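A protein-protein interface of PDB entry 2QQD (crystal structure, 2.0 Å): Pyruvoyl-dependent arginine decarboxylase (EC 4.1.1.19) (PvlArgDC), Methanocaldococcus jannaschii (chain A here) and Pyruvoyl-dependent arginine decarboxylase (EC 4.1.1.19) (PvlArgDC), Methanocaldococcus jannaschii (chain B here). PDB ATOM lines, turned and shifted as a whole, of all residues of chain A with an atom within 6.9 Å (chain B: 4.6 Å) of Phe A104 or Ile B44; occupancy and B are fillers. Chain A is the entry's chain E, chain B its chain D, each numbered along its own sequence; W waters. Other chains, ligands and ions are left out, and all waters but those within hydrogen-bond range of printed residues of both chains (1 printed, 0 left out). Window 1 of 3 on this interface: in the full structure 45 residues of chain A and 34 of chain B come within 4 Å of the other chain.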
ATOM      1  N   LEU A  11      15.186   1.014 -19.616  1.00  0.00           N
ATOM      2  CA  LEU A  11      15.387   1.169 -18.181  1.00  0.00           C
ATOM      3  C   LEU A  11      16.173  -0.019 -17.645  1.00  0.00           C
ATOM      4  O   LEU A  11      15.714  -1.156 -17.736  1.00  0.00           O
ATOM      5  CB  LEU A  11      14.040   1.256 -17.464  1.00  0.00           C
ATOM      6  CG  LEU A  11      14.162   1.507 -15.965  1.00  0.00           C
ATOM      7  CD1 LEU A  11      14.767   2.890 -15.743  1.00  0.00           C
ATOM      8  CD2 LEU A  11      12.796   1.398 -15.299  1.00  0.00           C
ATOM      9  N   LEU A  14      17.538  -1.308 -11.825  1.00  0.00           N
ATOM     10  CA  LEU A  14      17.980  -0.366 -10.808  1.00  0.00           C
ATOM     11  C   LEU A  14      18.065  -0.984  -9.424  1.00  0.00           C
ATOM     12  O   LEU A  14      17.161  -1.689  -8.988  1.00  0.00           O
ATOM     13  CB  LEU A  14      17.031   0.839 -10.757  1.00  0.00           C
ATOM     14  CG  LEU A  14      16.872   1.699 -12.017  1.00  0.00           C
ATOM     15  CD1 LEU A  14      15.762   2.719 -11.795  1.00  0.00           C
ATOM     16  CD2 LEU A  14      18.184   2.399 -12.345  1.00  0.00           C
ATOM     17  N   VAL A  20      17.949   8.110  -7.890  1.00  0.00           N
ATOM     18  CA  VAL A  20      17.952   8.290  -9.336  1.00  0.00           C
ATOM     19  C   VAL A  20      17.531   9.689  -9.804  1.00  0.00           C
ATOM     20  O   VAL A  20      16.391  10.099  -9.588  1.00  0.00           O
ATOM     21  CB  VAL A  20      16.993   7.245  -9.988  1.00  0.00           C
ATOM     22  CG1 VAL A  20      17.101   7.289 -11.501  1.00  0.00           C
ATOM     23  CG2 VAL A  20      17.297   5.845  -9.452  1.00  0.00           C
ATOM     24  N   THR A  22      15.921  12.237 -11.877  1.00  0.00           N
ATOM     25  CA  THR A  22      14.861  12.020 -12.842  1.00  0.00           C
ATOM     26  C   THR A  22      14.061  13.266 -13.159  1.00  0.00           C
ATOM     27  O   THR A  22      13.695  14.016 -12.265  1.00  0.00           O
ATOM     28  CB  THR A  22      13.879  10.953 -12.302  1.00  0.00           C
ATOM     29  OG1 THR A  22      14.621   9.836 -11.789  1.00  0.00           O
ATOM     30  CG2 THR A  22      12.941  10.469 -13.397  1.00  0.00           C
ATOM     31  N   ALA A  23      13.811  13.488 -14.445  1.00  0.00           N
ATOM     32  CA  ALA A  23      12.987  14.606 -14.878  1.00  0.00           C
ATOM     33  C   ALA A  23      11.647  13.913 -15.112  1.00  0.00           C
ATOM     34  O   ALA A  23      11.594  12.850 -15.736  1.00  0.00           O
ATOM     35  CB  ALA A  23      13.520  15.204 -16.179  1.00  0.00           C
ATOM     36  N   TYR A  24      10.567  14.474 -14.585  1.00  0.00           N
ATOM     37  CA  TYR A  24       9.278  13.833 -14.780  1.00  0.00           C
ATOM     38  C   TYR A  24       8.088  14.759 -14.680  1.00  0.00           C
ATOM     39  O   TYR A  24       8.176  15.873 -14.164  1.00  0.00           O
ATOM     40  CB  TYR A  24       9.103  12.673 -13.785  1.00  0.00           C
ATOM     41  CG  TYR A  24       9.055  13.068 -12.320  1.00  0.00           C
ATOM     42  CD1 TYR A  24       7.890  13.598 -11.751  1.00  0.00           C
ATOM     43  CD2 TYR A  24      10.162  12.873 -11.491  1.00  0.00           C
ATOM     44  CE1 TYR A  24       7.825  13.913 -10.392  1.00  0.00           C
ATOM     45  CE2 TYR A  24      10.112  13.187 -10.132  1.00  0.00           C
ATOM     46  CZ  TYR A  24       8.943  13.704  -9.587  1.00  0.00           C
ATOM     47  OH  TYR A  24       8.889  14.012  -8.242  1.00  0.00           O
ATOM     48  N   GLY A  25       6.969  14.262 -15.189  1.00  0.00           N
ATOM     49  CA  GLY A  25       5.725  14.997 -15.167  1.00  0.00           C
ATOM     50  C   GLY A  25       4.659  14.012 -14.746  1.00  0.00           C
ATOM     51  O   GLY A  25       4.707  12.837 -15.103  1.00  0.00           O
ATOM     52  N   TYR A  26       3.705  14.479 -13.962  1.00  0.00           N
ATOM     53  CA  TYR A  26       2.636  13.619 -13.510  1.00  0.00           C
ATOM     54  C   TYR A  26       1.428  14.493 -13.241  1.00  0.00           C
ATOM     55  O   TYR A  26       1.543  15.715 -13.112  1.00  0.00           O
ATOM     56  CB  TYR A  26       3.046  12.894 -12.228  1.00  0.00           C
ATOM     57  CG  TYR A  26       3.050  13.788 -11.016  1.00  0.00           C
ATOM     58  CD1 TYR A  26       1.978  13.786 -10.119  1.00  0.00           C
ATOM     59  CD2 TYR A  26       4.098  14.677 -10.790  1.00  0.00           C
ATOM     60  CE1 TYR A  26       1.954  14.651  -9.023  1.00  0.00           C
ATOM     61  CE2 TYR A  26       4.084  15.543  -9.705  1.00  0.00           C
ATOM     62  CZ  TYR A  26       3.009  15.524  -8.825  1.00  0.00           C
ATOM     63  OH  TYR A  26       3.001  16.376  -7.748  1.00  0.00           O
ATOM     64  N   ILE A  27       0.274  13.851 -13.159  1.00  0.00           N
ATOM     65  CA  ILE A  27      -0.976  14.531 -12.884  1.00  0.00           C
ATOM     66  C   ILE A  27      -1.836  13.530 -12.133  1.00  0.00           C
ATOM     67  O   ILE A  27      -1.879  12.348 -12.487  1.00  0.00           O
ATOM     68  CB  ILE A  27      -1.680  14.971 -14.193  1.00  0.00           C
ATOM     69  CG1 ILE A  27      -3.050  15.584 -13.871  1.00  0.00           C
ATOM     70  CG2 ILE A  27      -1.832  13.783 -15.133  1.00  0.00           C
ATOM     71  CD1 ILE A  27      -3.701  16.275 -15.062  1.00  0.00           C
ATOM     72  N   SER A  37      -3.272  12.539 -18.941  1.00  0.00           N
ATOM     73  CA  SER A  37      -2.064  12.056 -19.585  1.00  0.00           C
ATOM     74  C   SER A  37      -0.790  12.719 -19.103  1.00  0.00           C
ATOM     75  O   SER A  37      -0.807  13.806 -18.538  1.00  0.00           O
ATOM     76  CB  SER A  37      -2.170  12.236 -21.102  1.00  0.00           C
ATOM     77  OG  SER A  37      -3.038  11.277 -21.672  1.00  0.00           O
ATOM     78  N   ALA A  38       0.323  12.035 -19.339  1.00  0.00           N
ATOM     79  CA  ALA A  38       1.639  12.534 -18.972  1.00  0.00           C
ATOM     80  C   ALA A  38       2.564  12.082 -20.087  1.00  0.00           C
ATOM     81  O   ALA A  38       2.378  10.996 -20.640  1.00  0.00           O
ATOM     82  CB  ALA A  38       2.074  11.944 -17.636  1.00  0.00           C
ATOM     83  N   ALA A  39       3.539  12.915 -20.444  1.00  0.00           N
ATOM     84  CA  ALA A  39       4.466  12.567 -21.515  1.00  0.00           C
ATOM     85  C   ALA A  39       5.844  13.181 -21.318  1.00  0.00           C
ATOM     86  O   ALA A  39       5.992  14.216 -20.682  1.00  0.00           O
ATOM     87  CB  ALA A  39       3.895  12.992 -22.872  1.00  0.00           C
ATOM     88  N   ILE A  40       6.849  12.522 -21.877  1.00  0.00           N
ATOM     89  CA  ILE A  40       8.229  12.975 -21.779  1.00  0.00           C
ATOM     90  C   ILE A  40       8.872  12.939 -23.163  1.00  0.00           C
ATOM     91  O   ILE A  40       8.600  12.040 -23.966  1.00  0.00           O
ATOM     92  CB  ILE A  40       9.047  12.053 -20.824  1.00  0.00           C
ATOM     93  CG1 ILE A  40       8.862  12.497 -19.373  1.00  0.00           C
ATOM     94  CG2 ILE A  40      10.531  12.063 -21.205  1.00  0.00           C
ATOM     95  CD1 ILE A  40       9.601  13.773 -19.007  1.00  0.00           C
ATOM     96  N   ILE A  91       7.636   9.586 -25.098  1.00  0.00           N
ATOM     97  CA  ILE A  91       6.815   8.532 -24.527  1.00  0.00           C
ATOM     98  C   ILE A  91       5.649   9.202 -23.808  1.00  0.00           C
ATOM     99  O   ILE A  91       5.813  10.258 -23.195  1.00  0.00           O
ATOM    100  CB  ILE A  91       7.619   7.701 -23.511  1.00  0.00           C
ATOM    101  CG1 ILE A  91       6.729   6.644 -22.861  1.00  0.00           C
ATOM    102  CG2 ILE A  91       8.194   8.620 -22.438  1.00  0.00           C
ATOM    103  CD1 ILE A  91       7.491   5.703 -21.944  1.00  0.00           C
ATOM    104  N   ALA A  92       4.475   8.595 -23.892  1.00  0.00           N
ATOM    105  CA  ALA A  92       3.299   9.140 -23.231  1.00  0.00           C
ATOM    106  C   ALA A  92       2.458   7.997 -22.681  1.00  0.00           C
ATOM    107  O   ALA A  92       2.641   6.840 -23.054  1.00  0.00           O
ATOM    108  CB  ALA A  92       2.475   9.978 -24.214  1.00  0.00           C
ATOM    109  N   VAL A  93       1.543   8.335 -21.785  1.00  0.00           N
ATOM    110  CA  VAL A  93       0.659   7.360 -21.170  1.00  0.00           C
ATOM    111  C   VAL A  93      -0.611   8.106 -20.797  1.00  0.00           C
ATOM    112  O   VAL A  93      -0.563   9.294 -20.476  1.00  0.00           O
ATOM    113  CB  VAL A  93       1.285   6.765 -19.880  1.00  0.00           C
ATOM    114  CG1 VAL A  93       1.466   7.859 -18.839  1.00  0.00           C
ATOM    115  CG2 VAL A  93       0.408   5.646 -19.327  1.00  0.00           C
ATOM    116  N   HIS A  95      -4.456   7.724 -18.613  1.00  0.00           N
ATOM    117  CA  HIS A  95      -5.197   6.941 -17.642  1.00  0.00           C
ATOM    118  C   HIS A  95      -6.622   7.468 -17.515  1.00  0.00           C
ATOM    119  O   HIS A  95      -6.836   8.678 -17.413  1.00  0.00           O
ATOM    120  CB  HIS A  95      -4.499   7.039 -16.285  1.00  0.00           C
ATOM    121  CG  HIS A  95      -5.179   6.279 -15.192  1.00  0.00           C
ATOM    122  ND1 HIS A  95      -4.900   4.958 -14.919  1.00  0.00           N
ATOM    123  CD2 HIS A  95      -6.123   6.657 -14.299  1.00  0.00           C
ATOM    124  CE1 HIS A  95      -5.641   4.555 -13.902  1.00  0.00           C
ATOM    125  NE2 HIS A  95      -6.390   5.568 -13.506  1.00  0.00           N
ATOM    126  N   CYS A 102      -3.370   8.339 -11.295  1.00  0.00           N
ATOM    127  CA  CYS A 102      -2.218   9.173 -11.583  1.00  0.00           C
ATOM    128  C   CYS A 102      -1.562   8.721 -12.876  1.00  0.00           C
ATOM    129  O   CYS A 102      -1.386   7.524 -13.105  1.00  0.00           O
ATOM    130  CB  CYS A 102      -1.198   9.094 -10.440  1.00  0.00           C
ATOM    131  SG  CYS A 102       0.451   9.706 -10.910  1.00  0.00           S
ATOM    132  N   ALA A 103      -1.221   9.690 -13.722  1.00  0.00           N
ATOM    133  CA  ALA A 103      -0.541   9.434 -14.988  1.00  0.00           C
ATOM    134  C   ALA A 103       0.881   9.944 -14.759  1.00  0.00           C
ATOM    135  O   ALA A 103       1.061  11.055 -14.275  1.00  0.00           O
ATOM    136  CB  ALA A 103      -1.204  10.212 -16.109  1.00  0.00           C
ATOM    137  N   PHE A 104       1.879   9.150 -15.131  1.00  0.00           N
ATOM    138  CA  PHE A 104       3.273   9.521 -14.887  1.00  0.00           C
ATOM    139  C   PHE A 104       4.225   9.227 -16.055  1.00  0.00           C
ATOM    140  O   PHE A 104       4.162   8.163 -16.667  1.00  0.00           O
ATOM    141  CB  PHE A 104       3.728   8.770 -13.626  1.00  0.00           C
ATOM    142  CG  PHE A 104       5.181   8.918 -13.307  1.00  0.00           C
ATOM    143  CD1 PHE A 104       5.657  10.060 -12.674  1.00  0.00           C
ATOM    144  CD2 PHE A 104       6.074   7.899 -13.614  1.00  0.00           C
ATOM    145  CE1 PHE A 104       7.010  10.182 -12.342  1.00  0.00           C
ATOM    146  CE2 PHE A 104       7.423   8.010 -13.290  1.00  0.00           C
ATOM    147  CZ  PHE A 104       7.891   9.154 -12.651  1.00  0.00           C
ATOM    148  N   ALA A 105       5.110  10.174 -16.364  1.00  0.00           N
ATOM    149  CA  ALA A 105       6.090   9.982 -17.436  1.00  0.00           C
ATOM    150  C   ALA A 105       7.438  10.489 -16.930  1.00  0.00           C
ATOM    151  O   ALA A 105       7.498  11.477 -16.198  1.00  0.00           O
ATOM    152  CB  ALA A 105       5.665  10.739 -18.699  1.00  0.00           C
ATOM    153  N   ALA A 106       8.524   9.827 -17.318  1.00  0.00           N
ATOM    154  CA  ALA A 106       9.831  10.243 -16.830  1.00  0.00           C
ATOM    155  C   ALA A 106      11.020   9.853 -17.697  1.00  0.00           C
ATOM    156  O   ALA A 106      10.947   8.939 -18.520  1.00  0.00           O
ATOM    157  CB  ALA A 106      10.042   9.699 -15.425  1.00  0.00           C
ATOM    158  N   ALA A 107      12.107  10.591 -17.498  1.00  0.00           N
ATOM    159  CA  ALA A 107      13.376  10.368 -18.178  1.00  0.00           C
ATOM    160  C   ALA A 107      14.312  10.113 -17.002  1.00  0.00           C
ATOM    161  O   ALA A 107      14.737  11.039 -16.318  1.00  0.00           O
ATOM    162  CB  ALA A 107      13.815  11.620 -18.946  1.00  0.00           C
ATOM    163  N   ALA A 108      14.595   8.848 -16.743  1.00  0.00           N
ATOM    164  CA  ALA A 108      15.460   8.497 -15.627  1.00  0.00           C
ATOM    165  C   ALA A 108      16.909   8.456 -16.095  1.00  0.00           C
ATOM    166  O   ALA A 108      17.247   7.762 -17.050  1.00  0.00           O
ATOM    167  CB  ALA A 108      15.047   7.144 -15.061  1.00  0.00           C
ATOM    168  N   VAL B  22      10.410   6.263 -19.391  1.00  0.00           N
ATOM    169  CA  VAL B  22       9.424   5.341 -18.845  1.00  0.00           C
ATOM    170  C   VAL B  22       8.134   6.093 -18.551  1.00  0.00           C
ATOM    171  O   VAL B  22       8.125   7.315 -18.441  1.00  0.00           O
ATOM    172  CB  VAL B  22       9.912   4.653 -17.536  1.00  0.00           C
ATOM    173  CG1 VAL B  22      11.189   3.854 -17.809  1.00  0.00           C
ATOM    174  CG2 VAL B  22      10.148   5.699 -16.450  1.00  0.00           C
ATOM    175  N   ALA B  23       7.045   5.353 -18.424  1.00  0.00           N
ATOM    176  CA  ALA B  23       5.759   5.957 -18.148  1.00  0.00           C
ATOM    177  C   ALA B  23       4.840   4.873 -17.625  1.00  0.00           C
ATOM    178  O   ALA B  23       5.015   3.689 -17.936  1.00  0.00           O
ATOM    179  CB  ALA B  23       5.184   6.573 -19.418  1.00  0.00           C
ATOM    180  N   GLY B  24       3.869   5.285 -16.824  1.00  0.00           N
ATOM    181  CA  GLY B  24       2.927   4.342 -16.260  1.00  0.00           C
ATOM    182  C   GLY B  24       1.841   5.119 -15.556  1.00  0.00           C
ATOM    183  O   GLY B  24       1.923   6.338 -15.436  1.00  0.00           O
ATOM    184  N   PHE B  35       0.327   7.839  -6.949  1.00  0.00           N
ATOM    185  CA  PHE B  35       1.616   8.235  -7.513  1.00  0.00           C
ATOM    186  C   PHE B  35       2.592   7.043  -7.414  1.00  0.00           C
ATOM    187  O   PHE B  35       3.248   6.678  -8.394  1.00  0.00           O
ATOM    188  CB  PHE B  35       2.157   9.434  -6.730  1.00  0.00           C
ATOM    189  CG  PHE B  35       3.467   9.962  -7.241  1.00  0.00           C
ATOM    190  CD1 PHE B  35       3.519  10.736  -8.399  1.00  0.00           C
ATOM    191  CD2 PHE B  35       4.648   9.692  -6.562  1.00  0.00           C
ATOM    192  CE1 PHE B  35       4.733  11.236  -8.874  1.00  0.00           C
ATOM    193  CE2 PHE B  35       5.872  10.184  -7.029  1.00  0.00           C
ATOM    194  CZ  PHE B  35       5.912  10.962  -8.190  1.00  0.00           C
ATOM    195  N   ALA B  38       1.890   4.382  -9.895  1.00  0.00           N
ATOM    196  CA  ALA B  38       2.278   4.776 -11.243  1.00  0.00           C
ATOM    197  C   ALA B  38       3.781   4.567 -11.455  1.00  0.00           C
ATOM    198  O   ALA B  38       4.203   4.037 -12.486  1.00  0.00           O
ATOM    199  CB  ALA B  38       1.912   6.223 -11.474  1.00  0.00           C
ATOM    200  N   LEU B  39       4.588   4.988 -10.485  1.00  0.00           N
ATOM    201  CA  LEU B  39       6.032   4.806 -10.600  1.00  0.00           C
ATOM    202  C   LEU B  39       6.286   3.311 -10.718  1.00  0.00           C
ATOM    203  O   LEU B  39       7.085   2.870 -11.543  1.00  0.00           O
ATOM    204  CB  LEU B  39       6.770   5.345  -9.371  1.00  0.00           C
ATOM    205  CG  LEU B  39       6.599   6.803  -8.930  1.00  0.00           C
ATOM    206  CD1 LEU B  39       7.899   7.243  -8.251  1.00  0.00           C
ATOM    207  CD2 LEU B  39       6.300   7.718 -10.104  1.00  0.00           C
ATOM    208  N   ALA B  42       5.484   2.081 -13.974  1.00  0.00           N
ATOM    209  CA  ALA B  42       6.505   2.583 -14.893  1.00  0.00           C
ATOM    210  C   ALA B  42       7.862   1.914 -14.682  1.00  0.00           C
ATOM    211  O   ALA B  42       8.765   2.062 -15.507  1.00  0.00           O
ATOM    212  CB  ALA B  42       6.654   4.092 -14.737  1.00  0.00           C
ATOM    213  N   GLY B  43       8.017   1.209 -13.565  1.00  0.00           N
ATOM    214  CA  GLY B  43       9.274   0.528 -13.304  1.00  0.00           C
ATOM    215  C   GLY B  43      10.278   1.241 -12.411  1.00  0.00           C
ATOM    216  O   GLY B  43      11.373   0.720 -12.196  1.00  0.00           O
ATOM    217  N   ILE B  44       9.939   2.421 -11.897  1.00  0.00           N
ATOM    218  CA  ILE B  44      10.852   3.149 -11.014  1.00  0.00           C
ATOM    219  C   ILE B  44      10.200   3.449  -9.673  1.00  0.00           C
ATOM    220  O   ILE B  44      10.460   4.483  -9.059  1.00  0.00           O
ATOM    221  CB  ILE B  44      11.324   4.491 -11.627  1.00  0.00           C
ATOM    222  CG1 ILE B  44      10.115   5.331 -12.048  1.00  0.00           C
ATOM    223  CG2 ILE B  44      12.263   4.232 -12.801  1.00  0.00           C
ATOM    224  CD1 ILE B  44      10.487   6.707 -12.546  1.00  0.00           C
ATOM    225  N   GLY B  45       9.354   2.532  -9.217  1.00  0.00           N
ATOM    226  CA  GLY B  45       8.670   2.726  -7.950  1.00  0.00           C
ATOM    227  C   GLY B  45       9.452   2.230  -6.748  1.00  0.00           C
ATOM    228  O   GLY B  45       9.055   2.480  -5.611  1.00  0.00           O
ATOM    229  N   ASN B  46      10.563   1.538  -6.990  1.00  0.00           N
ATOM    230  CA  ASN B  46      11.378   1.017  -5.893  1.00  0.00           C
ATOM    231  C   ASN B  46      12.748   1.690  -5.773  1.00  0.00           C
ATOM    232  O   ASN B  46      13.725   1.068  -5.343  1.00  0.00           O
ATOM    233  CB  ASN B  46      11.524  -0.501  -6.034  1.00  0.00           C
ATOM    234  CG  ASN B  46      10.239  -1.241  -5.686  1.00  0.00           C
ATOM    235  OD1 ASN B  46       9.909  -2.264  -6.290  1.00  0.00           O
ATOM    236  ND2 ASN B  46       9.515  -0.729  -4.698  1.00  0.00           N
ATOM    237  N   VAL B  47      12.796   2.962  -6.172  1.00  0.00           N
ATOM    238  CA  VAL B  47      13.995   3.791  -6.085  1.00  0.00           C
ATOM    239  C   VAL B  47      13.575   5.170  -5.588  1.00  0.00           C
ATOM    240  O   VAL B  47      12.401   5.543  -5.659  1.00  0.00           O
ATOM    241  CB  VAL B  47      14.708   3.997  -7.465  1.00  0.00           C
ATOM    242  CG1 VAL B  47      15.413   2.717  -7.907  1.00  0.00           C
ATOM    243  CG2 VAL B  47      13.694   4.447  -8.513  1.00  0.00           C
ATOM    244  N   LEU B  49      13.595   8.919  -6.224  1.00  0.00           N
ATOM    245  CA  LEU B  49      13.777   9.850  -7.318  1.00  0.00           C
ATOM    246  C   LEU B  49      14.229  11.235  -6.878  1.00  0.00           C
ATOM    247  O   LEU B  49      13.604  11.856  -6.020  1.00  0.00           O
ATOM    248  CB  LEU B  49      12.477   9.995  -8.105  1.00  0.00           C
ATOM    249  CG  LEU B  49      11.836   8.732  -8.695  1.00  0.00           C
ATOM    250  CD1 LEU B  49      10.575   9.140  -9.451  1.00  0.00           C
ATOM    251  CD2 LEU B  49      12.797   8.025  -9.629  1.00  0.00           C
HETATM  252  O   HOH W   1      14.662  -0.863  -7.837  1.00  0.00           O
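N of Ala A106 is in hydrogen-bond range of O of Val B22, at 2.8 Å. O of Gly B24 lies within hydrogen-bond range of N of Phe A104 (2.8 Å).
O of Leu B39 lies within hydrogen-bond range of N of Ile B44 (2.9 Å). The side-chain hydroxyl (OG1) of Thr A22 is in hydrogen-bond range of the backbone carbonyl oxygen (O) of Val A20, 2.8 Å away. O of Gly A25 lies within hydrogen-bond range of N of Ala A105 (3.0 Å). The side-chain hydroxyl (OG) of Ser A37 sits close to the backbone carbonyl oxygen (O) of Val A93 (3.4 Å). The backbone NH (N) of Val A93 sits at hydrogen-bond distance from the backbone carbonyl oxygen (O) of Ala A38 (3.0 Å). The backbone NH (N) of Ile A40 is in hydrogen-bond range of the backbone carbonyl oxygen (O) of Ile A91 (2.8 Å).
Among the printed residues, merely in contact across the chains: Phe A104 with Ala B23, Phe A104 with Leu B39, Thr A22 with Leu B49, Phe A104 with Ile B44, Val A20 with Leu B49, Ile A91 with Val B22, Leu A11 with Gly B43, Ala A105 with Val B22, Ile A91 with Ala B23, Tyr A26 with Phe B35, Val A20 with Val B47, Val A93 with Gly B24, Leu A14 with Val B47, Phe A104 with Ala B38, Ala A103 with Gly B24, Leu A11 with Ile B44, Cys A102 with Ala B38, Leu A11 with Val B22, Cys A102 with Phe B35, Val A93 with Ala B23 and Leu A14 with Ile B44.
Of the printed residues of chain B, Phe A104 touches Ala B23, Gly B24, Ala B38, Leu B39 and Ile B44. Printed residues of chain A within 4 Å of Ile B44: Leu A11, Leu A14 and Phe A104. Of chain A, only Leu A11 comes within 4 Å of Gly B43. Printed residues of chain A within 4 Å of Ala B23: Ile A91, Val A93 and Phe A104. Of the printed residues of chain B, Tyr A26 touches Phe B35. Printed residues of chain A within 4 Å of Val B22: Leu A11 (3.9 Å), Ile A91 (3.5 Å), Ala A105 (3.5 Å) and Ala A106 (2.8 Å). Ala A108 touches none of the printed residues of chain B. The nearest printed residue of chain B that does not touch Phe A104 is Ala B42 (4.01 Å). The nearest residue of chain A that does not touch Ile B44 is Ala A106 (4.2 Å).
Of the 24 printed residues of chain A, 12 touch a printed residue of chain B. Hydrophobic or aromatic side chains of chain A within 4 Å of the printed part of chain B: Leu A11, Leu A14, Val A20, Tyr A26, Ile A91, Val A93 and Phe A104. Along chain A the printed residues that touch a printed residue of chain B span positions 11 to 106. Of the 13 printed residues of chain B, 10 touch a printed residue of chain A. Printed residues of chain B that touch a printed residue of chain A: Val B22, Ala B23, Gly B24, Phe B35, Ala B38, Leu B39, Gly B43, Ile B44, Val B47 and Leu B49.
Water W1 bridges O of Leu A14 and O of Asn B46.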
